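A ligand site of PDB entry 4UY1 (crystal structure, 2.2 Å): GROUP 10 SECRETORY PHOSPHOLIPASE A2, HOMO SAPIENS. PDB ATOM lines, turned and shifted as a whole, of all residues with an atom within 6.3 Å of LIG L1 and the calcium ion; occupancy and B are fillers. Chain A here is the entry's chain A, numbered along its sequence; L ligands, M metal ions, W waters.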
ATOM      1  N   ILE A   2      12.349   3.287   0.650  1.00  0.00           N
ATOM      2  CA  ILE A   2      11.277   3.578  -0.286  1.00  0.00           C
ATOM      3  C   ILE A   2      10.052   2.685  -0.043  1.00  0.00           C
ATOM      4  O   ILE A   2       8.924   3.109  -0.261  1.00  0.00           O
ATOM      5  CB  ILE A   2      11.748   3.483  -1.765  1.00  0.00           C
ATOM      6  CG1 ILE A   2      12.936   4.421  -2.069  1.00  0.00           C
ATOM      7  CG2 ILE A   2      10.634   3.864  -2.746  1.00  0.00           C
ATOM      8  CD1 ILE A   2      12.776   5.856  -1.585  1.00  0.00           C
ATOM      9  N   LEU A   5       8.258   4.343   2.747  1.00  0.00           N
ATOM     10  CA  LEU A   5       7.729   5.625   2.225  1.00  0.00           C
ATOM     11  C   LEU A   5       6.408   5.428   1.451  1.00  0.00           C
ATOM     12  O   LEU A   5       5.423   6.152   1.647  1.00  0.00           O
ATOM     13  CB  LEU A   5       8.789   6.297   1.330  1.00  0.00           C
ATOM     14  CG  LEU A   5       8.411   7.520   0.513  1.00  0.00           C
ATOM     15  CD1 LEU A   5       7.902   8.623   1.427  1.00  0.00           C
ATOM     16  CD2 LEU A   5       9.592   8.027  -0.312  1.00  0.00           C
ATOM     17  N   ALA A   6       6.400   4.441   0.569  1.00  0.00           N
ATOM     18  CA  ALA A   6       5.176   4.060  -0.164  1.00  0.00           C
ATOM     19  C   ALA A   6       4.045   3.710   0.812  1.00  0.00           C
ATOM     20  O   ALA A   6       2.946   4.290   0.749  1.00  0.00           O
ATOM     21  CB  ALA A   6       5.468   2.891  -1.085  1.00  0.00           C
ATOM     22  N   VAL A   9       2.673   6.719   3.101  1.00  0.00           N
ATOM     23  CA  VAL A   9       1.916   7.696   2.272  1.00  0.00           C
ATOM     24  C   VAL A   9       0.528   7.154   1.906  1.00  0.00           C
ATOM     25  O   VAL A   9      -0.453   7.874   1.971  1.00  0.00           O
ATOM     26  CB  VAL A   9       2.740   8.081   1.018  1.00  0.00           C
ATOM     27  CG1 VAL A   9       1.923   8.791  -0.066  1.00  0.00           C
ATOM     28  CG2 VAL A   9       3.939   8.937   1.441  1.00  0.00           C
ATOM     29  N   PRO A  17       0.686   6.206  -4.328  1.00  0.00           N
ATOM     30  CA  PRO A  17       2.024   6.814  -4.253  1.00  0.00           C
ATOM     31  C   PRO A  17       2.608   7.184  -5.627  1.00  0.00           C
ATOM     32  O   PRO A  17       3.499   8.022  -5.712  1.00  0.00           O
ATOM     33  CB  PRO A  17       2.879   5.735  -3.574  1.00  0.00           C
ATOM     34  CG  PRO A  17       1.899   4.813  -2.918  1.00  0.00           C
ATOM     35  CD  PRO A  17       0.672   4.833  -3.774  1.00  0.00           C
ATOM     36  N   ILE A  18       2.099   6.566  -6.692  1.00  0.00           N
ATOM     37  CA  ILE A  18       2.445   6.905  -8.093  1.00  0.00           C
ATOM     38  C   ILE A  18       2.216   8.396  -8.427  1.00  0.00           C
ATOM     39  O   ILE A  18       2.909   8.964  -9.268  1.00  0.00           O
ATOM     40  CB  ILE A  18       1.647   6.012  -9.089  1.00  0.00           C
ATOM     41  CG1 ILE A  18       2.084   4.545  -8.975  1.00  0.00           C
ATOM     42  CG2 ILE A  18       1.816   6.469 -10.542  1.00  0.00           C
ATOM     43  CD1 ILE A  18       1.068   3.569  -9.545  1.00  0.00           C
ATOM     44  N   TYR A  20       2.989  10.949  -6.816  1.00  0.00           N
ATOM     45  CA  TYR A  20       4.056  11.813  -6.319  1.00  0.00           C
ATOM     46  C   TYR A  20       5.403  11.522  -6.919  1.00  0.00           C
ATOM     47  O   TYR A  20       6.436  11.972  -6.382  1.00  0.00           O
ATOM     48  CB  TYR A  20       4.164  11.657  -4.803  1.00  0.00           C
ATOM     49  CG  TYR A  20       2.859  11.918  -4.085  1.00  0.00           C
ATOM     50  CD1 TYR A  20       2.305  13.190  -4.105  1.00  0.00           C
ATOM     51  CD2 TYR A  20       2.163  10.896  -3.426  1.00  0.00           C
ATOM     52  CE1 TYR A  20       1.090  13.451  -3.470  1.00  0.00           C
ATOM     53  CE2 TYR A  20       0.966  11.154  -2.765  1.00  0.00           C
ATOM     54  CZ  TYR A  20       0.428  12.423  -2.796  1.00  0.00           C
ATOM     55  OH  TYR A  20      -0.751  12.703  -2.168  1.00  0.00           O
ATOM     56  N   MET A  21       5.426  10.751  -8.002  1.00  0.00           N
ATOM     57  CA  MET A  21       6.708  10.245  -8.516  1.00  0.00           C
ATOM     58  C   MET A  21       7.410  11.247  -9.474  1.00  0.00           C
ATOM     59  O   MET A  21       8.637  11.355  -9.444  1.00  0.00           O
ATOM     60  CB  MET A  21       6.582   8.803  -9.049  1.00  0.00           C
ATOM     61  CG  MET A  21       6.535   7.766  -7.903  1.00  0.00           C
ATOM     62  SD  MET A  21       6.501   6.006  -8.313  1.00  0.00           S
ATOM     63  CE  MET A  21       8.157   5.782  -8.951  1.00  0.00           C
ATOM     64  N   CYS A  25       8.121  20.762  -8.976  1.00  0.00           N
ATOM     65  CA  CYS A  25       9.557  20.949  -9.040  1.00  0.00           C
ATOM     66  C   CYS A  25      10.371  20.072  -8.037  1.00  0.00           C
ATOM     67  O   CYS A  25      11.590  19.887  -8.203  1.00  0.00           O
ATOM     68  CB  CYS A  25       9.864  22.463  -8.862  1.00  0.00           C
ATOM     69  SG  CYS A  25       9.285  23.479 -10.282  1.00  0.00           S
ATOM     70  N   PHE A  26       9.695  19.521  -7.020  1.00  0.00           N
ATOM     71  CA  PHE A  26      10.400  18.754  -5.989  1.00  0.00           C
ATOM     72  C   PHE A  26      10.013  17.282  -5.857  1.00  0.00           C
ATOM     73  O   PHE A  26      10.836  16.481  -5.413  1.00  0.00           O
ATOM     74  CB  PHE A  26      10.342  19.485  -4.633  1.00  0.00           C
ATOM     75  CG  PHE A  26      11.176  20.745  -4.611  1.00  0.00           C
ATOM     76  CD1 PHE A  26      10.634  21.956  -5.012  1.00  0.00           C
ATOM     77  CD2 PHE A  26      12.523  20.717  -4.208  1.00  0.00           C
ATOM     78  CE1 PHE A  26      11.403  23.125  -5.057  1.00  0.00           C
ATOM     79  CE2 PHE A  26      13.288  21.884  -4.223  1.00  0.00           C
ATOM     80  CZ  PHE A  26      12.729  23.087  -4.648  1.00  0.00           C
ATOM     81  N   CYS A  27       8.796  16.898  -6.217  1.00  0.00           N
ATOM     82  CA  CYS A  27       8.354  15.517  -5.977  1.00  0.00           C
ATOM     83  C   CYS A  27       8.989  14.549  -6.975  1.00  0.00           C
ATOM     84  O   CYS A  27       8.683  14.589  -8.149  1.00  0.00           O
ATOM     85  CB  CYS A  27       6.839  15.391  -5.986  1.00  0.00           C
ATOM     86  SG  CYS A  27       5.988  16.367  -4.720  1.00  0.00           S
ATOM     87  N   GLY A  28       9.892  13.711  -6.479  1.00  0.00           N
ATOM     88  CA  GLY A  28      10.659  12.782  -7.305  1.00  0.00           C
ATOM     89  C   GLY A  28      12.131  12.984  -7.012  1.00  0.00           C
ATOM     90  O   GLY A  28      12.502  13.802  -6.156  1.00  0.00           O
ATOM     91  N   LEU A  29      12.986  12.264  -7.718  1.00  0.00           N
ATOM     92  CA  LEU A  29      14.441  12.309  -7.511  1.00  0.00           C
ATOM     93  C   LEU A  29      14.983  13.720  -7.759  1.00  0.00           C
ATOM     94  O   LEU A  29      14.801  14.287  -8.828  1.00  0.00           O
ATOM     95  CB  LEU A  29      15.102  11.266  -8.403  1.00  0.00           C
ATOM     96  CG  LEU A  29      16.617  11.068  -8.329  1.00  0.00           C
ATOM     97  CD1 LEU A  29      17.085  10.721  -6.921  1.00  0.00           C
ATOM     98  CD2 LEU A  29      17.049  10.005  -9.324  1.00  0.00           C
ATOM     99  N   GLY A  30      15.623  14.295  -6.745  1.00  0.00           N
ATOM    100  CA  GLY A  30      16.133  15.664  -6.801  1.00  0.00           C
ATOM    101  C   GLY A  30      15.050  16.718  -6.686  1.00  0.00           C
ATOM    102  O   GLY A  30      13.976  16.477  -6.109  1.00  0.00           O
ATOM    103  N   GLY A  31      15.334  17.891  -7.263  1.00  0.00           N
ATOM    104  CA  GLY A  31      14.380  18.995  -7.276  1.00  0.00           C
ATOM    105  C   GLY A  31      15.026  20.326  -6.946  1.00  0.00           C
ATOM    106  O   GLY A  31      15.876  20.406  -6.085  1.00  0.00           O
ATOM    107  N   CYS A  42       5.440  19.934   0.533  1.00  0.00           N
ATOM    108  CA  CYS A  42       5.613  18.683   1.296  1.00  0.00           C
ATOM    109  C   CYS A  42       6.862  17.916   0.855  1.00  0.00           C
ATOM    110  O   CYS A  42       7.615  17.409   1.697  1.00  0.00           O
ATOM    111  CB  CYS A  42       4.398  17.789   1.155  1.00  0.00           C
ATOM    112  SG  CYS A  42       2.858  18.462   1.874  1.00  0.00           S
ATOM    113  N   CYS A  43       7.062  17.838  -0.470  1.00  0.00           N
ATOM    114  CA  CYS A  43       8.198  17.164  -1.058  1.00  0.00           C
ATOM    115  C   CYS A  43       9.541  17.910  -0.857  1.00  0.00           C
ATOM    116  O   CYS A  43      10.575  17.282  -0.665  1.00  0.00           O
ATOM    117  CB  CYS A  43       7.941  16.914  -2.538  1.00  0.00           C
ATOM    118  SG  CYS A  43       6.658  15.706  -2.953  1.00  0.00           S
ATOM    119  N   HIS A  44       9.523  19.243  -0.909  1.00  0.00           N
ATOM    120  CA  HIS A  44      10.720  20.013  -0.537  1.00  0.00           C
ATOM    121  C   HIS A  44      11.151  19.718   0.910  1.00  0.00           C
ATOM    122  O   HIS A  44      12.315  19.442   1.174  1.00  0.00           O
ATOM    123  CB  HIS A  44      10.473  21.518  -0.744  1.00  0.00           C
ATOM    124  CG  HIS A  44      11.560  22.389  -0.187  1.00  0.00           C
ATOM    125  ND1 HIS A  44      11.552  22.857   1.114  1.00  0.00           N
ATOM    126  CD2 HIS A  44      12.700  22.853  -0.747  1.00  0.00           C
ATOM    127  CE1 HIS A  44      12.631  23.579   1.318  1.00  0.00           C
ATOM    128  NE2 HIS A  44      13.345  23.590   0.217  1.00  0.00           N
ATOM    129  N   HIS A  46      10.408  17.001   2.694  1.00  0.00           N
ATOM    130  CA  HIS A  46      10.882  15.618   2.769  1.00  0.00           C
ATOM    131  C   HIS A  46      12.315  15.496   2.211  1.00  0.00           C
ATOM    132  O   HIS A  46      13.148  14.805   2.796  1.00  0.00           O
ATOM    133  CB  HIS A  46       9.935  14.689   1.989  1.00  0.00           C
ATOM    134  CG  HIS A  46      10.104  13.227   2.283  1.00  0.00           C
ATOM    135  ND1 HIS A  46      10.419  12.295   1.317  1.00  0.00           N
ATOM    136  CD2 HIS A  46       9.918  12.511   3.433  1.00  0.00           C
ATOM    137  CE1 HIS A  46      10.449  11.093   1.853  1.00  0.00           C
ATOM    138  NE2 HIS A  46      10.147  11.199   3.133  1.00  0.00           N
ATOM    139  N   ASP A  47      12.565  16.155   1.078  1.00  0.00           N
ATOM    140  CA  ASP A  47      13.923  16.267   0.512  1.00  0.00           C
ATOM    141  C   ASP A  47      14.940  16.745   1.572  1.00  0.00           C
ATOM    142  O   ASP A  47      16.042  16.203   1.662  1.00  0.00           O
ATOM    143  CB  ASP A  47      13.960  17.238  -0.684  1.00  0.00           C
ATOM    144  CG  ASP A  47      13.325  16.677  -1.953  1.00  0.00           C
ATOM    145  OD1 ASP A  47      12.727  15.586  -1.934  1.00  0.00           O
ATOM    146  OD2 ASP A  47      13.416  17.362  -3.020  1.00  0.00           O
ATOM    147  N   TYR A  50      15.423  14.006   4.435  1.00  0.00           N
ATOM    148  CA  TYR A  50      16.296  12.937   3.930  1.00  0.00           C
ATOM    149  C   TYR A  50      17.750  13.417   3.834  1.00  0.00           C
ATOM    150  O   TYR A  50      18.664  12.634   4.072  1.00  0.00           O
ATOM    151  CB  TYR A  50      15.789  12.401   2.555  1.00  0.00           C
ATOM    152  CG  TYR A  50      14.824  11.216   2.626  1.00  0.00           C
ATOM    153  CD1 TYR A  50      14.022  10.987   3.766  1.00  0.00           C
ATOM    154  CD2 TYR A  50      14.674  10.347   1.536  1.00  0.00           C
ATOM    155  CE1 TYR A  50      13.128   9.908   3.805  1.00  0.00           C
ATOM    156  CE2 TYR A  50      13.796   9.265   1.563  1.00  0.00           C
ATOM    157  CZ  TYR A  50      13.016   9.045   2.696  1.00  0.00           C
ATOM    158  OH  TYR A  50      12.130   7.974   2.726  1.00  0.00           O
ATOM    159  N   ILE A  94       5.887  13.574   5.818  1.00  0.00           N
ATOM    160  CA  ILE A  94       5.427  13.788   4.455  1.00  0.00           C
ATOM    161  C   ILE A  94       4.036  13.173   4.242  1.00  0.00           C
ATOM    162  O   ILE A  94       3.179  13.793   3.591  1.00  0.00           O
ATOM    163  CB  ILE A  94       6.449  13.357   3.356  1.00  0.00           C
ATOM    164  CG1 ILE A  94       6.073  14.032   2.044  1.00  0.00           C
ATOM    165  CG2 ILE A  94       6.558  11.839   3.220  1.00  0.00           C
ATOM    166  CD1 ILE A  94       6.709  13.432   0.800  1.00  0.00           C
ATOM    167  N   LEU A  98       0.984  15.434   2.950  1.00  0.00           N
ATOM    168  CA  LEU A  98       0.320  15.165   1.687  1.00  0.00           C
ATOM    169  C   LEU A  98      -1.154  14.792   1.833  1.00  0.00           C
ATOM    170  O   LEU A  98      -1.975  15.137   0.972  1.00  0.00           O
ATOM    171  CB  LEU A  98       1.057  14.048   0.938  1.00  0.00           C
ATOM    172  CG  LEU A  98       2.483  14.368   0.481  1.00  0.00           C
ATOM    173  CD1 LEU A  98       3.218  13.112   0.058  1.00  0.00           C
ATOM    174  CD2 LEU A  98       2.452  15.383  -0.664  1.00  0.00           C
HETATM  175  C1  LIG L   1       6.775   5.751  -3.437  1.00  0.00           C
HETATM  176  C2  LIG L   1       6.755   7.173  -3.084  1.00  0.00           C
HETATM  177  C3  LIG L   1       7.703   8.122  -3.412  1.00  0.00           C
HETATM  178  C4  LIG L   1       7.391   9.415  -2.913  1.00  0.00           C
HETATM  179  C5  LIG L   1       6.199   9.466  -2.210  1.00  0.00           C
HETATM  180  C6  LIG L   1       5.581  10.619  -1.563  1.00  0.00           C
HETATM  181  S1  LIG L   1       5.491   7.888  -2.149  1.00  0.00           S
HETATM  182  C7  LIG L   1       8.309  10.505  -3.180  1.00  0.00           C
HETATM  183  C8  LIG L   1       8.662  11.551  -2.284  1.00  0.00           C
HETATM  184  C9  LIG L   1       9.586  12.284  -2.987  1.00  0.00           C
HETATM  185  N1  LIG L   1       9.705  11.655  -4.198  1.00  0.00           N
HETATM  186  N2  LIG L   1       8.951  10.560  -4.342  1.00  0.00           N
HETATM  187  C10 LIG L   1      10.346  13.450  -2.699  1.00  0.00           C
HETATM  188  O1  LIG L   1      10.937  14.046  -3.585  1.00  0.00           O
HETATM  189  N3  LIG L   1      10.380  13.862  -1.377  1.00  0.00           N
HETATM  190  O1  LG2 L   2      14.974  14.148  -3.672  1.00  0.00           O
HETATM  191  C1  LG2 L   2      15.292  12.788  -3.353  1.00  0.00           C
HETATM  192  C2  LG2 L   2      14.026  11.948  -3.561  1.00  0.00           C
HETATM  193  O2  LG2 L   2      13.449  11.492  -2.311  1.00  0.00           O
HETATM  194  C3  LG2 L   2      12.395   9.387  -3.026  1.00  0.00           C
HETATM  195  C4  LG2 L   2      13.402  10.072  -2.119  1.00  0.00           C
HETATM  196  O3  LG2 L   2      13.039   8.992  -4.243  1.00  0.00           O
HETATM  197  C5  LG2 L   2      14.802   7.789  -5.400  1.00  0.00           C
HETATM  198  C6  LG2 L   2      13.650   7.693  -4.363  1.00  0.00           C
HETATM  199  O4  LG2 L   2      15.429   6.530  -5.713  1.00  0.00           O
HETATM  200  C7  LG2 L   2      17.664   7.547  -5.969  1.00  0.00           C
HETATM  201  C8  LG2 L   2      16.828   6.386  -5.434  1.00  0.00           C
HETATM  202  O5  LG2 L   2      19.043   7.335  -5.631  1.00  0.00           O
HETATM  203  C9  LG2 L   2      19.815   9.454  -4.740  1.00  0.00           C
HETATM  204  C10 LG2 L   2      19.539   7.979  -4.472  1.00  0.00           C
HETATM  205  O6  LG2 L   2      20.358   9.979  -3.520  1.00  0.00           O
HETATM  206 CA    CA M   1      12.733  15.424  -4.472  1.00  0.00          CA
HETATM  207  O   HOH W   1       9.408   8.732  -6.281  1.00  0.00           O
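SG of Cys 27 is disulfide-bonded to SG of Cys 43, at 2.0 Å. N of Leu 98 sits at hydrogen-bond distance from SG of Cys 42 (3.7 Å).
A nitrogen (N1) of LIG L1 sits at hydrogen-bond distance from the backbone NH (N) of Gly 28. A nitrogen (N3) of LIG L1 sits at hydrogen-bond distance from a ring nitrogen (ND1) of His 46, 3.1 Å away. O of Cys 43 lies within hydrogen-bond range of N3 of LIG L1, at 3.5 Å.
The calcium ion is bound by the backbone carbonyl oxygen (O) of Gly 30 (2.3 Å), the backbone carbonyl oxygen (O) of Gly 28 (2.3 Å), the backbone carbonyl oxygen (O) of Phe 26 (2.4 Å), an oxygen (O1) of LIG L1 (2.4 Å), the side-chain carboxylate (OD2) of Asp 47 (2.5 Å), the side-chain carboxylate (OD1) of Asp 47 (2.5 Å) and an oxygen (O1) of LG2 L2 (2.7 Å).
Within 4 Å of the calcium ion: Phe 26, Gly 28, Gly 30 and Asp 47.
CD2 of Leu 5 touches C3 of LIG L1, 3.6 Å away. CB of Ala 6 touches C1 of LIG L1 (3.9 Å). Val 9 touches LIG L1. CB of Pro 17 touches S1 of LIG L1 (3.7 Å). Tyr 20 touches LIG L1 (O to N2, 3.5 Å). Cys 27 touches LIG L1 (CA to O1, 3.8 Å). Ile 94 touches LIG L1 (CD1 to C6, 3.8 Å). Leu 98 touches LIG L1 (CD1 to C6, 3.8 Å). Hydrophobic or aromatic side chains within 4 Å of LIG L1: Leu 5, Ala 6, Val 9, Pro 17, Tyr 20, His 46, Ile 94 and Leu 98. Of the 23 residues printed, 13 come within 4 Å of LIG L1.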
